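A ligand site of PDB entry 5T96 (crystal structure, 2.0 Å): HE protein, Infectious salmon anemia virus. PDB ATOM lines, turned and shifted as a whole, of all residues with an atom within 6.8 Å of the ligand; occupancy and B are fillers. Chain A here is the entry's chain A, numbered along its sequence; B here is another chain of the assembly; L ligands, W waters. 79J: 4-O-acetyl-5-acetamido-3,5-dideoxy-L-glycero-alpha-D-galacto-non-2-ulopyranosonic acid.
The side-chain carboxylate of Asp 125 sits at hydrogen-bond distance from an oxygen (O9) of the ligand (3.0 Å). The backbone NH of Asp 125 is in hydrogen-bond range of an oxygen (O9) of the ligand. An oxygen (O1B) of the ligand is in salt-bridge range of the guanidinium group of Arg 123 (2.7 Å). The side-chain hydroxyl of Thr 124 sits close to an oxygen (O9) of the ligand, 3.2 Å away. NH1 of Arg 182 of chain B lies within hydrogen-bond range of O2 of the ligand, at 2.8 Å. O of Arg 123 is in hydrogen-bond range of N5 of the ligand. An oxygen (O) of the ligand is in hydrogen-bond range of the backbone NH of Arg 123 (3.1 Å).
O of Val 144 of chain B sits at hydrogen-bond distance from N of Gly 114 of chain B (2.8 Å). The side-chain hydroxyl (OG1) of Thr 136 sits at hydrogen-bond distance from the side-chain amide nitrogen (NE2) of Gln 189 (3.1 Å). O of Ile 142 of chain B is in hydrogen-bond range of N of Ala 116 of chain B (2.9 Å). The side-chain hydroxyl of Thr 124 lies within hydrogen-bond range of the backbone NH of Ala 126 (2.9 Å). The backbone carbonyl oxygen of Leu 181 of chain B is in hydrogen-bond range of the guanidinium group of Arg 123 (3.3 Å). N of Val 134 sits at hydrogen-bond distance from O of Gly 122 (2.8 Å). The backbone carbonyl oxygen (O) of Val 121 lies within hydrogen-bond range of the backbone NH (N) of Ala 115 of chain B, 3.0 Å away.
Gly 122 touches the ligand. Gln 189 touches the ligand (NE2 to C11, 3.9 Å). Ala 115 of chain B touches the ligand (C to CH3, 3.2 Å). N of Ala 116 of chain B touches CH3 of the ligand (3.4 Å). Val 144 of chain B touches the ligand. Hydrophobic or aromatic side chains within 4 Å of the ligand: Val 144 of chain B. Within 4 Å of the ligand: Gly 122, Arg 123, Thr 124, Asp 125, Gln 189, Ala 115 of chain B, Ala 116 of chain B, Val 144 of chain B and Arg 182 of chain B. Along chain A the residues within 4 Å of the ligand span positions 122 to 189.
Water W4 bridges OG of Ser 131 (2.6 Å) and O1A of the ligand (3.0 Å).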
ATOM      1  N   LEU A 120      -9.017 -12.685  31.772  1.00  0.00           N
ATOM      2  CA  LEU A 120      -8.378 -13.562  30.810  1.00  0.00           C
ATOM      3  C   LEU A 120      -7.041 -12.946  30.367  1.00  0.00           C
ATOM      4  O   LEU A 120      -7.025 -11.845  29.811  1.00  0.00           O
ATOM      5  CB  LEU A 120      -9.292 -13.748  29.629  1.00  0.00           C
ATOM      6  CG  LEU A 120      -8.837 -14.681  28.528  1.00  0.00           C
ATOM      7  CD1 LEU A 120      -8.693 -16.119  29.041  1.00  0.00           C
ATOM      8  CD2 LEU A 120      -9.883 -14.574  27.437  1.00  0.00           C
ATOM      9  N   VAL A 121      -5.935 -13.663  30.583  1.00  0.00           N
ATOM     10  CA  VAL A 121      -4.607 -13.202  30.178  1.00  0.00           C
ATOM     11  C   VAL A 121      -4.333 -13.549  28.728  1.00  0.00           C
ATOM     12  O   VAL A 121      -4.343 -14.724  28.334  1.00  0.00           O
ATOM     13  CB  VAL A 121      -3.510 -13.810  31.060  1.00  0.00           C
ATOM     14  CG1 VAL A 121      -2.134 -13.312  30.586  1.00  0.00           C
ATOM     15  CG2 VAL A 121      -3.696 -13.442  32.522  1.00  0.00           C
ATOM     16  N   GLY A 122      -3.969 -12.532  27.943  1.00  0.00           N
ATOM     17  CA  GLY A 122      -3.624 -12.728  26.555  1.00  0.00           C
ATOM     18  C   GLY A 122      -2.743 -11.598  26.079  1.00  0.00           C
ATOM     19  O   GLY A 122      -2.290 -10.764  26.873  1.00  0.00           O
ATOM     20  N   ARG A 123      -2.500 -11.569  24.775  1.00  0.00           N
ATOM     21  CA  ARG A 123      -1.750 -10.494  24.154  1.00  0.00           C
ATOM     22  C   ARG A 123      -2.557 -10.023  22.954  1.00  0.00           C
ATOM     23  O   ARG A 123      -3.289 -10.803  22.345  1.00  0.00           O
ATOM     24  CB  ARG A 123      -0.337 -10.938  23.688  1.00  0.00           C
ATOM     25  CG  ARG A 123      -0.383 -11.928  22.565  1.00  0.00           C
ATOM     26  CD  ARG A 123       1.003 -12.467  22.182  1.00  0.00           C
ATOM     27  NE  ARG A 123       0.963 -13.282  20.974  1.00  0.00           N
ATOM     28  CZ  ARG A 123       1.849 -14.238  20.693  1.00  0.00           C
ATOM     29  NH1 ARG A 123       2.830 -14.494  21.521  1.00  0.00           N
ATOM     30  NH2 ARG A 123       1.731 -14.929  19.577  1.00  0.00           N
ATOM     31  N   THR A 124      -2.421  -8.737  22.627  1.00  0.00           N
ATOM     32  CA  THR A 124      -3.150  -8.193  21.505  1.00  0.00           C
ATOM     33  C   THR A 124      -2.482  -6.913  21.059  1.00  0.00           C
ATOM     34  O   THR A 124      -1.838  -6.219  21.856  1.00  0.00           O
ATOM     35  CB  THR A 124      -4.621  -7.895  21.865  1.00  0.00           C
ATOM     36  OG1 THR A 124      -5.350  -7.452  20.715  1.00  0.00           O
ATOM     37  CG2 THR A 124      -4.692  -6.817  22.923  1.00  0.00           C
ATOM     38  N   ASP A 125      -2.682  -6.576  19.784  1.00  0.00           N
ATOM     39  CA  ASP A 125      -2.310  -5.268  19.262  1.00  0.00           C
ATOM     40  C   ASP A 125      -3.512  -4.346  19.194  1.00  0.00           C
ATOM     41  O   ASP A 125      -3.398  -3.240  18.660  1.00  0.00           O
ATOM     42  CB  ASP A 125      -1.641  -5.405  17.897  1.00  0.00           C
ATOM     43  CG  ASP A 125      -2.524  -6.073  16.870  1.00  0.00           C
ATOM     44  OD1 ASP A 125      -3.746  -6.187  17.099  1.00  0.00           O
ATOM     45  OD2 ASP A 125      -2.008  -6.478  15.819  1.00  0.00           O
ATOM     46  N   ALA A 126      -4.668  -4.757  19.741  1.00  0.00           N
ATOM     47  CA  ALA A 126      -5.881  -3.950  19.594  1.00  0.00           C
ATOM     48  C   ALA A 126      -5.901  -2.738  20.505  1.00  0.00           C
ATOM     49  O   ALA A 126      -6.662  -1.794  20.243  1.00  0.00           O
ATOM     50  CB  ALA A 126      -7.120  -4.785  19.906  1.00  0.00           C
ATOM     51  N   PHE A 130       0.312  -2.331  18.733  1.00  0.00           N
ATOM     52  CA  PHE A 130       1.361  -3.340  18.708  1.00  0.00           C
ATOM     53  C   PHE A 130       1.134  -4.291  19.888  1.00  0.00           C
ATOM     54  O   PHE A 130       0.374  -4.000  20.806  1.00  0.00           O
ATOM     55  CB  PHE A 130       2.744  -2.688  18.774  1.00  0.00           C
ATOM     56  CG  PHE A 130       2.821  -1.681  19.855  1.00  0.00           C
ATOM     57  CD1 PHE A 130       3.125  -2.064  21.150  1.00  0.00           C
ATOM     58  CD2 PHE A 130       2.525  -0.357  19.585  1.00  0.00           C
ATOM     59  CE1 PHE A 130       3.153  -1.118  22.165  1.00  0.00           C
ATOM     60  CE2 PHE A 130       2.550   0.581  20.572  1.00  0.00           C
ATOM     61  CZ  PHE A 130       2.863   0.184  21.877  1.00  0.00           C
ATOM     62  N   SER A 131       1.814  -5.433  19.850  1.00  0.00           N
ATOM     63  CA  SER A 131       1.462  -6.535  20.739  1.00  0.00           C
ATOM     64  C   SER A 131       1.919  -6.240  22.165  1.00  0.00           C
ATOM     65  O   SER A 131       3.096  -5.940  22.409  1.00  0.00           O
ATOM     66  CB  SER A 131       2.084  -7.826  20.195  1.00  0.00           C
ATOM     67  OG  SER A 131       1.646  -8.944  20.936  1.00  0.00           O
ATOM     68  N   VAL A 134      -2.433  -8.161  27.821  1.00  0.00           N
ATOM     69  CA  VAL A 134      -3.645  -7.578  28.376  1.00  0.00           C
ATOM     70  C   VAL A 134      -4.415  -8.582  29.218  1.00  0.00           C
ATOM     71  O   VAL A 134      -4.216  -9.798  29.136  1.00  0.00           O
ATOM     72  CB  VAL A 134      -4.582  -7.048  27.296  1.00  0.00           C
ATOM     73  CG1 VAL A 134      -3.872  -5.951  26.524  1.00  0.00           C
ATOM     74  CG2 VAL A 134      -4.968  -8.169  26.377  1.00  0.00           C
ATOM     75  N   THR A 136      -8.453  -9.399  29.530  1.00  0.00           N
ATOM     76  CA  THR A 136      -9.763  -9.190  28.921  1.00  0.00           C
ATOM     77  C   THR A 136     -10.860  -9.524  29.927  1.00  0.00           C
ATOM     78  O   THR A 136     -10.873 -10.625  30.500  1.00  0.00           O
ATOM     79  CB  THR A 136      -9.922 -10.044  27.661  1.00  0.00           C
ATOM     80  OG1 THR A 136      -8.859  -9.753  26.739  1.00  0.00           O
ATOM     81  CG2 THR A 136     -11.293  -9.766  26.988  1.00  0.00           C
ATOM     82  N   GLN A 189     -10.502  -4.463  27.625  1.00  0.00           N
ATOM     83  CA  GLN A 189      -9.121  -4.882  27.760  1.00  0.00           C
ATOM     84  C   GLN A 189      -8.305  -3.803  28.440  1.00  0.00           C
ATOM     85  O   GLN A 189      -8.534  -2.598  28.233  1.00  0.00           O
ATOM     86  CB  GLN A 189      -8.530  -5.224  26.400  1.00  0.00           C
ATOM     87  CG  GLN A 189      -9.192  -6.439  25.744  1.00  0.00           C
ATOM     88  CD  GLN A 189      -8.629  -6.799  24.359  1.00  0.00           C
ATOM     89  OE1 GLN A 189      -8.383  -5.935  23.511  1.00  0.00           O
ATOM     90  NE2 GLN A 189      -8.388  -8.080  24.145  1.00  0.00           N
ATOM     91  N   PHE B 112       6.076 -13.406  29.302  1.00  0.00           N
ATOM     92  CA  PHE B 112       4.636 -13.367  29.074  1.00  0.00           C
ATOM     93  C   PHE B 112       4.140 -14.729  28.632  1.00  0.00           C
ATOM     94  O   PHE B 112       4.743 -15.393  27.777  1.00  0.00           O
ATOM     95  CB  PHE B 112       4.271 -12.347  28.018  1.00  0.00           C
ATOM     96  CG  PHE B 112       2.885 -12.562  27.486  1.00  0.00           C
ATOM     97  CD1 PHE B 112       1.795 -12.199  28.264  1.00  0.00           C
ATOM     98  CD2 PHE B 112       2.671 -13.189  26.271  1.00  0.00           C
ATOM     99  CE1 PHE B 112       0.534 -12.417  27.836  1.00  0.00           C
ATOM    100  CE2 PHE B 112       1.396 -13.420  25.817  1.00  0.00           C
ATOM    101  CZ  PHE B 112       0.312 -13.037  26.599  1.00  0.00           C
ATOM    102  N   GLY B 114       0.036 -16.461  27.889  1.00  0.00           N
ATOM    103  CA  GLY B 114      -1.400 -16.301  27.954  1.00  0.00           C
ATOM    104  C   GLY B 114      -2.089 -17.347  27.113  1.00  0.00           C
ATOM    105  O   GLY B 114      -1.447 -18.229  26.540  1.00  0.00           O
ATOM    106  N   ALA B 115      -3.416 -17.244  27.039  1.00  0.00           N
ATOM    107  CA  ALA B 115      -4.207 -18.255  26.361  1.00  0.00           C
ATOM    108  C   ALA B 115      -5.616 -17.734  26.160  1.00  0.00           C
ATOM    109  O   ALA B 115      -6.013 -16.728  26.742  1.00  0.00           O
ATOM    110  CB  ALA B 115      -4.214 -19.564  27.157  1.00  0.00           C
ATOM    111  N   ALA B 116      -6.370 -18.440  25.302  1.00  0.00           N
ATOM    112  CA  ALA B 116      -7.748 -18.076  24.983  1.00  0.00           C
ATOM    113  C   ALA B 116      -8.723 -18.484  26.071  1.00  0.00           C
ATOM    114  O   ALA B 116      -9.875 -18.021  26.036  1.00  0.00           O
ATOM    115  CB  ALA B 116      -8.187 -18.731  23.684  1.00  0.00           C
ATOM    116  N   ILE B 117      -8.307 -19.342  27.004  1.00  0.00           N
ATOM    117  CA  ILE B 117      -9.045 -19.665  28.208  1.00  0.00           C
ATOM    118  C   ILE B 117      -8.090 -19.483  29.387  1.00  0.00           C
ATOM    119  O   ILE B 117      -6.877 -19.374  29.218  1.00  0.00           O
ATOM    120  CB  ILE B 117      -9.613 -21.102  28.176  1.00  0.00           C
ATOM    121  CG1 ILE B 117      -8.466 -22.122  28.066  1.00  0.00           C
ATOM    122  CG2 ILE B 117     -10.641 -21.247  27.035  1.00  0.00           C
ATOM    123  CD1 ILE B 117      -8.896 -23.558  28.053  1.00  0.00           C
ATOM    124  N   THR B 141      -6.846 -25.198  23.453  1.00  0.00           N
ATOM    125  CA  THR B 141      -6.957 -23.746  23.369  1.00  0.00           C
ATOM    126  C   THR B 141      -5.740 -23.175  22.627  1.00  0.00           C
ATOM    127  O   THR B 141      -4.787 -23.891  22.284  1.00  0.00           O
ATOM    128  CB  THR B 141      -7.070 -23.132  24.773  1.00  0.00           C
ATOM    129  OG1 THR B 141      -7.432 -21.762  24.670  1.00  0.00           O
ATOM    130  CG2 THR B 141      -5.771 -23.208  25.548  1.00  0.00           C
ATOM    131  N   ILE B 142      -5.817 -21.881  22.360  1.00  0.00           N
ATOM    132  CA  ILE B 142      -4.706 -21.094  21.850  1.00  0.00           C
ATOM    133  C   ILE B 142      -3.845 -20.668  23.035  1.00  0.00           C
ATOM    134  O   ILE B 142      -4.343 -20.013  23.963  1.00  0.00           O
ATOM    135  CB  ILE B 142      -5.210 -19.861  21.092  1.00  0.00           C
ATOM    136  CG1 ILE B 142      -6.037 -20.270  19.882  1.00  0.00           C
ATOM    137  CG2 ILE B 142      -4.061 -19.013  20.639  1.00  0.00           C
ATOM    138  CD1 ILE B 142      -6.819 -19.139  19.317  1.00  0.00           C
ATOM    139  N   VAL B 143      -2.553 -20.985  22.964  1.00  0.00           N
ATOM    140  CA  VAL B 143      -1.561 -20.612  23.976  1.00  0.00           C
ATOM    141  C   VAL B 143      -0.534 -19.685  23.329  1.00  0.00           C
ATOM    142  O   VAL B 143      -0.040 -19.961  22.229  1.00  0.00           O
ATOM    143  CB  VAL B 143      -0.865 -21.846  24.583  1.00  0.00           C
ATOM    144  CG1 VAL B 143       0.200 -21.446  25.550  1.00  0.00           C
ATOM    145  CG2 VAL B 143      -1.875 -22.795  25.262  1.00  0.00           C
ATOM    146  N   VAL B 144      -0.208 -18.571  24.012  1.00  0.00           N
ATOM    147  CA  VAL B 144       0.729 -17.583  23.495  1.00  0.00           C
ATOM    148  C   VAL B 144       1.834 -17.363  24.520  1.00  0.00           C
ATOM    149  O   VAL B 144       1.574 -17.350  25.721  1.00  0.00           O
ATOM    150  CB  VAL B 144       0.054 -16.244  23.143  1.00  0.00           C
ATOM    151  CG1 VAL B 144      -0.738 -16.374  21.878  1.00  0.00           C
ATOM    152  CG2 VAL B 144      -0.862 -15.747  24.303  1.00  0.00           C
ATOM    153  N   ASN B 148       6.193  -9.706  20.628  1.00  0.00           N
ATOM    154  CA  ASN B 148       6.911  -9.066  19.533  1.00  0.00           C
ATOM    155  C   ASN B 148       7.853  -8.009  20.086  1.00  0.00           C
ATOM    156  O   ASN B 148       7.488  -7.268  21.005  1.00  0.00           O
ATOM    157  CB  ASN B 148       5.940  -8.402  18.542  1.00  0.00           C
ATOM    158  CG  ASN B 148       5.161  -9.411  17.696  1.00  0.00           C
ATOM    159  OD1 ASN B 148       5.554 -10.570  17.569  1.00  0.00           O
ATOM    160  ND2 ASN B 148       4.031  -8.971  17.133  1.00  0.00           N
ATOM    161  N   LEU B 181       5.841 -17.110  20.501  1.00  0.00           N
ATOM    162  CA  LEU B 181       5.303 -18.273  19.831  1.00  0.00           C
ATOM    163  C   LEU B 181       3.805 -18.387  20.104  1.00  0.00           C
ATOM    164  O   LEU B 181       3.254 -17.734  20.996  1.00  0.00           O
ATOM    165  CB  LEU B 181       6.096 -19.537  20.230  1.00  0.00           C
ATOM    166  CG  LEU B 181       6.131 -19.989  21.680  1.00  0.00           C
ATOM    167  CD1 LEU B 181       4.768 -20.409  22.157  1.00  0.00           C
ATOM    168  CD2 LEU B 181       7.108 -21.135  21.853  1.00  0.00           C
ATOM    169  N   ARG B 182       3.130 -19.171  19.260  1.00  0.00           N
ATOM    170  CA  ARG B 182       1.715 -19.446  19.382  1.00  0.00           C
ATOM    171  C   ARG B 182       1.494 -20.936  19.144  1.00  0.00           C
ATOM    172  O   ARG B 182       1.930 -21.467  18.116  1.00  0.00           O
ATOM    173  CB  ARG B 182       0.901 -18.628  18.382  1.00  0.00           C
ATOM    174  CG  ARG B 182      -0.542 -19.098  18.239  1.00  0.00           C
ATOM    175  CD  ARG B 182      -1.309 -18.205  17.330  1.00  0.00           C
ATOM    176  NE  ARG B 182      -2.562 -18.813  16.955  1.00  0.00           N
ATOM    177  CZ  ARG B 182      -3.677 -18.139  16.682  1.00  0.00           C
ATOM    178  NH1 ARG B 182      -3.702 -16.820  16.764  1.00  0.00           N
ATOM    179  NH2 ARG B 182      -4.761 -18.800  16.321  1.00  0.00           N
HETATM  180  C1  79J L   1      -1.299 -13.420  18.562  1.00  0.00           C
HETATM  181  C10 79J L   1      -6.585 -12.378  22.039  1.00  0.00           C
HETATM  182  C11 79J L   1      -6.918 -11.547  23.280  1.00  0.00           C
HETATM  183  O1A 79J L   1      -1.044 -12.398  19.231  1.00  0.00           O
HETATM  184  C2  79J L   1      -2.730 -13.718  18.245  1.00  0.00           C
HETATM  185  C3  79J L   1      -3.286 -14.674  19.310  1.00  0.00           C
HETATM  186  C4  79J L   1      -3.855 -13.982  20.553  1.00  0.00           C
HETATM  187  O4  79J L   1      -4.489 -14.944  21.338  1.00  0.00           O
HETATM  188  C5  79J L   1      -4.902 -12.948  20.176  1.00  0.00           C
HETATM  189  C6  79J L   1      -4.205 -11.960  19.254  1.00  0.00           C
HETATM  190  C7  79J L   1      -5.258 -10.979  18.685  1.00  0.00           C
HETATM  191  C8  79J L   1      -4.745 -10.251  17.442  1.00  0.00           C
HETATM  192  C9  79J L   1      -3.304  -9.816  17.573  1.00  0.00           C
HETATM  193  O10 79J L   1      -7.357 -13.205  21.674  1.00  0.00           O
HETATM  194  N5  79J L   1      -5.337 -12.200  21.345  1.00  0.00           N
HETATM  195  C   79J L   1      -4.331 -14.848  22.714  1.00  0.00           C
HETATM  196  O   79J L   1      -3.726 -13.938  23.189  1.00  0.00           O
HETATM  197  CH3 79J L   1      -4.907 -15.964  23.559  1.00  0.00           C
HETATM  198  O1B 79J L   1      -0.412 -14.224  18.086  1.00  0.00           O
HETATM  199  O2  79J L   1      -2.543 -14.301  16.962  1.00  0.00           O
HETATM  200  O6  79J L   1      -3.498 -12.547  18.183  1.00  0.00           O
HETATM  201  O7  79J L   1      -6.457 -11.615  18.323  1.00  0.00           O
HETATM  202  O8  79J L   1      -5.471  -9.050  17.347  1.00  0.00           O
HETATM  203  O9  79J L   1      -3.478  -8.803  18.488  1.00  0.00           O
HETATM  204  O   HOH W   1      -8.516 -14.536  23.827  1.00  0.00           O
HETATM  205  O   HOH W   2      -9.032 -10.788  20.034  1.00  0.00           O
HETATM  206  O   HOH W   3       1.425 -15.492  15.913  1.00  0.00           O
HETATM  207  O   HOH W   4      -0.511  -9.445  19.506  1.00  0.00           O
